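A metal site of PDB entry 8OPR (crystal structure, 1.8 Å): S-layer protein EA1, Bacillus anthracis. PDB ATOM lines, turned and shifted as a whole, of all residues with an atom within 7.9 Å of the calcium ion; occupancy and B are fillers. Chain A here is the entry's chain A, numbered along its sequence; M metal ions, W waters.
The side-chain carboxylate of Glu 356 sits close to the backbone NH of Val 371 (2.9 Å).
Of the 14 residues printed, 4 come within 4 Å of the calcium ion.
The calcium ion is bound by the side-chain carboxylate (OD1) of Asp 370 (2.2 Å), the backbone carbonyl oxygen (O) of Ile 354 (2.4 Å), water W2 (2.4 Å), the backbone carbonyl oxygen (O) of Thr 351 (2.5 Å), the side-chain carboxylate (OE2) of Glu 356 (2.6 Å), the side-chain carboxylate (OE1) of Glu 356 (2.6 Å) and water W1 (2.6 Å).
Water W1 bridges O of Val 371 (2.5 Å) and O of Asn 350 (2.7 Å).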
ATOM      1  N   ALA A 349     -23.525  21.635 -20.198  1.00  0.00           N
ATOM      2  CA  ALA A 349     -22.268  20.932 -20.299  1.00  0.00           C
ATOM      3  C   ALA A 349     -22.377  19.754 -21.264  1.00  0.00           C
ATOM      4  O   ALA A 349     -23.237  18.891 -21.095  1.00  0.00           O
ATOM      5  CB  ALA A 349     -21.835  20.466 -18.926  1.00  0.00           C
ATOM      6  N   ASN A 350     -21.522  19.747 -22.280  1.00  0.00           N
ATOM      7  CA  ASN A 350     -21.525  18.656 -23.235  1.00  0.00           C
ATOM      8  C   ASN A 350     -20.551  17.550 -22.732  1.00  0.00           C
ATOM      9  O   ASN A 350     -20.009  17.662 -21.622  1.00  0.00           O
ATOM     10  CB  ASN A 350     -21.203  19.181 -24.672  1.00  0.00           C
ATOM     11  CG  ASN A 350     -19.837  19.786 -24.839  1.00  0.00           C
ATOM     12  OD1 ASN A 350     -19.037  19.829 -23.910  1.00  0.00           O
ATOM     13  ND2 ASN A 350     -19.550  20.317 -26.014  1.00  0.00           N
ATOM     14  N   THR A 351     -20.312  16.502 -23.547  1.00  0.00           N
ATOM     15  CA  THR A 351     -19.417  15.413 -23.151  1.00  0.00           C
ATOM     16  C   THR A 351     -18.034  15.895 -22.750  1.00  0.00           C
ATOM     17  O   THR A 351     -17.513  15.459 -21.722  1.00  0.00           O
ATOM     18  CB  THR A 351     -19.317  14.373 -24.289  1.00  0.00           C
ATOM     19  OG1 THR A 351     -20.587  13.746 -24.451  1.00  0.00           O
ATOM     20  CG2 THR A 351     -18.236  13.316 -24.047  1.00  0.00           C
ATOM     21  N   ALA A 352     -17.472  16.837 -23.524  1.00  0.00           N
ATOM     22  CA  ALA A 352     -16.104  17.283 -23.244  1.00  0.00           C
ATOM     23  C   ALA A 352     -15.986  18.254 -22.069  1.00  0.00           C
ATOM     24  O   ALA A 352     -14.905  18.383 -21.534  1.00  0.00           O
ATOM     25  CB  ALA A 352     -15.479  17.867 -24.489  1.00  0.00           C
ATOM     26  N   ALA A 353     -17.074  18.908 -21.662  1.00  0.00           N
ATOM     27  CA  ALA A 353     -17.037  19.905 -20.593  1.00  0.00           C
ATOM     28  C   ALA A 353     -16.650  19.319 -19.219  1.00  0.00           C
ATOM     29  O   ALA A 353     -15.980  19.977 -18.432  1.00  0.00           O
ATOM     30  CB  ALA A 353     -18.376  20.635 -20.498  1.00  0.00           C
ATOM     31  N   ILE A 354     -17.117  18.097 -18.939  1.00  0.00           N
ATOM     32  CA  ILE A 354     -16.836  17.464 -17.655  1.00  0.00           C
ATOM     33  C   ILE A 354     -16.086  16.154 -17.872  1.00  0.00           C
ATOM     34  O   ILE A 354     -16.504  15.315 -18.669  1.00  0.00           O
ATOM     35  CB  ILE A 354     -18.150  17.215 -16.840  1.00  0.00           C
ATOM     36  CG1 ILE A 354     -18.927  18.516 -16.627  1.00  0.00           C
ATOM     37  CG2 ILE A 354     -17.826  16.559 -15.497  1.00  0.00           C
ATOM     38  CD1 ILE A 354     -20.347  18.310 -16.177  1.00  0.00           C
ATOM     39  N   LYS A 355     -14.963  15.997 -17.176  1.00  0.00           N
ATOM     40  CA  LYS A 355     -14.198  14.770 -17.215  1.00  0.00           C
ATOM     41  C   LYS A 355     -14.585  14.028 -15.936  1.00  0.00           C
ATOM     42  O   LYS A 355     -14.365  14.532 -14.832  1.00  0.00           O
ATOM     43  CB  LYS A 355     -12.680  15.011 -17.255  1.00  0.00           C
ATOM     44  CG  LYS A 355     -12.260  16.396 -17.749  1.00  0.00           C
ATOM     45  CD  LYS A 355     -11.773  16.417 -19.198  1.00  0.00           C
ATOM     46  CE  LYS A 355     -12.889  16.161 -20.177  1.00  0.00           C
ATOM     47  NZ  LYS A 355     -12.606  16.799 -21.489  1.00  0.00           N
ATOM     48  N   GLU A 356     -15.231  12.866 -16.120  1.00  0.00           N
ATOM     49  CA  GLU A 356     -15.673  12.097 -14.972  1.00  0.00           C
ATOM     50  C   GLU A 356     -14.549  11.154 -14.553  1.00  0.00           C
ATOM     51  O   GLU A 356     -14.330  10.124 -15.181  1.00  0.00           O
ATOM     52  CB  GLU A 356     -17.014  11.388 -15.283  1.00  0.00           C
ATOM     53  CG  GLU A 356     -18.144  12.357 -15.664  1.00  0.00           C
ATOM     54  CD  GLU A 356     -18.202  12.856 -17.105  1.00  0.00           C
ATOM     55  OE1 GLU A 356     -17.425  12.331 -17.940  1.00  0.00           O
ATOM     56  OE2 GLU A 356     -19.011  13.762 -17.401  1.00  0.00           O
ATOM     57  N   LEU A 369     -20.461   6.869 -16.739  1.00  0.00           N
ATOM     58  CA  LEU A 369     -21.018   8.133 -16.284  1.00  0.00           C
ATOM     59  C   LEU A 369     -20.537   9.317 -17.106  1.00  0.00           C
ATOM     60  O   LEU A 369     -19.369   9.687 -17.032  1.00  0.00           O
ATOM     61  CB  LEU A 369     -20.803   8.354 -14.773  1.00  0.00           C
ATOM     62  CG  LEU A 369     -21.380   9.650 -14.158  1.00  0.00           C
ATOM     63  CD1 LEU A 369     -22.875   9.784 -14.425  1.00  0.00           C
ATOM     64  CD2 LEU A 369     -21.140   9.688 -12.640  1.00  0.00           C
ATOM     65  N   ASP A 370     -21.404   9.875 -17.935  1.00  0.00           N
ATOM     66  CA  ASP A 370     -21.093  11.065 -18.733  1.00  0.00           C
ATOM     67  C   ASP A 370     -22.167  12.121 -18.393  1.00  0.00           C
ATOM     68  O   ASP A 370     -23.306  11.959 -18.781  1.00  0.00           O
ATOM     69  CB  ASP A 370     -21.079  10.760 -20.250  1.00  0.00           C
ATOM     70  CG  ASP A 370     -20.492  11.887 -21.119  1.00  0.00           C
ATOM     71  OD1 ASP A 370     -19.747  12.741 -20.577  1.00  0.00           O
ATOM     72  OD2 ASP A 370     -20.787  11.917 -22.318  1.00  0.00           O
ATOM     73  N   VAL A 371     -21.823  13.126 -17.590  1.00  0.00           N
ATOM     74  CA  VAL A 371     -22.758  14.189 -17.190  1.00  0.00           C
ATOM     75  C   VAL A 371     -22.966  15.211 -18.320  1.00  0.00           C
ATOM     76  O   VAL A 371     -22.118  16.085 -18.532  1.00  0.00           O
ATOM     77  CB  VAL A 371     -22.256  14.905 -15.911  1.00  0.00           C
ATOM     78  CG1 VAL A 371     -23.302  15.912 -15.409  1.00  0.00           C
ATOM     79  CG2 VAL A 371     -21.853  13.896 -14.814  1.00  0.00           C
ATOM     80  N   VAL A 372     -24.066  15.046 -19.099  1.00  0.00           N
ATOM     81  CA  VAL A 372     -24.439  15.858 -20.240  1.00  0.00           C
ATOM     82  C   VAL A 372     -25.746  16.565 -19.915  1.00  0.00           C
ATOM     83  O   VAL A 372     -26.718  15.965 -19.451  1.00  0.00           O
ATOM     84  CB  VAL A 372     -24.430  15.091 -21.575  1.00  0.00           C
ATOM     85  CG1 VAL A 372     -24.793  16.023 -22.728  1.00  0.00           C
ATOM     86  CG2 VAL A 372     -23.064  14.468 -21.817  1.00  0.00           C
ATOM     87  N   PHE A 398     -15.551  15.265 -10.600  1.00  0.00           N
ATOM     88  CA  PHE A 398     -15.933  15.915 -11.849  1.00  0.00           C
ATOM     89  C   PHE A 398     -14.920  17.004 -12.100  1.00  0.00           C
ATOM     90  O   PHE A 398     -14.767  17.881 -11.263  1.00  0.00           O
ATOM     91  CB  PHE A 398     -17.356  16.488 -11.720  1.00  0.00           C
ATOM     92  CG  PHE A 398     -18.340  15.410 -11.379  1.00  0.00           C
ATOM     93  CD1 PHE A 398     -18.492  14.299 -12.196  1.00  0.00           C
ATOM     94  CD2 PHE A 398     -19.085  15.470 -10.214  1.00  0.00           C
ATOM     95  CE1 PHE A 398     -19.370  13.287 -11.856  1.00  0.00           C
ATOM     96  CE2 PHE A 398     -19.979  14.443  -9.884  1.00  0.00           C
ATOM     97  CZ  PHE A 398     -20.103  13.362 -10.702  1.00  0.00           C
ATOM     98  N   GLN A 399     -14.166  16.898 -13.191  1.00  0.00           N
ATOM     99  CA  GLN A 399     -13.133  17.892 -13.480  1.00  0.00           C
ATOM    100  C   GLN A 399     -13.373  18.646 -14.786  1.00  0.00           C
ATOM    101  O   GLN A 399     -14.105  18.174 -15.643  1.00  0.00           O
ATOM    102  CB  GLN A 399     -11.756  17.199 -13.508  1.00  0.00           C
ATOM    103  CG  GLN A 399     -11.365  16.536 -12.202  1.00  0.00           C
ATOM    104  CD  GLN A 399      -9.918  16.057 -12.237  1.00  0.00           C
ATOM    105  OE1 GLN A 399      -9.297  15.883 -13.295  1.00  0.00           O
ATOM    106  NE2 GLN A 399      -9.371  15.826 -11.057  1.00  0.00           N
HETATM  107 CA    CA M   1     -18.119  14.002 -19.780  1.00  0.00          CA
HETATM  108  O   HOH W   1     -19.863  15.914 -19.618  1.00  0.00           O
HETATM  109  O   HOH W   2     -16.216  12.905 -20.864  1.00  0.00           O
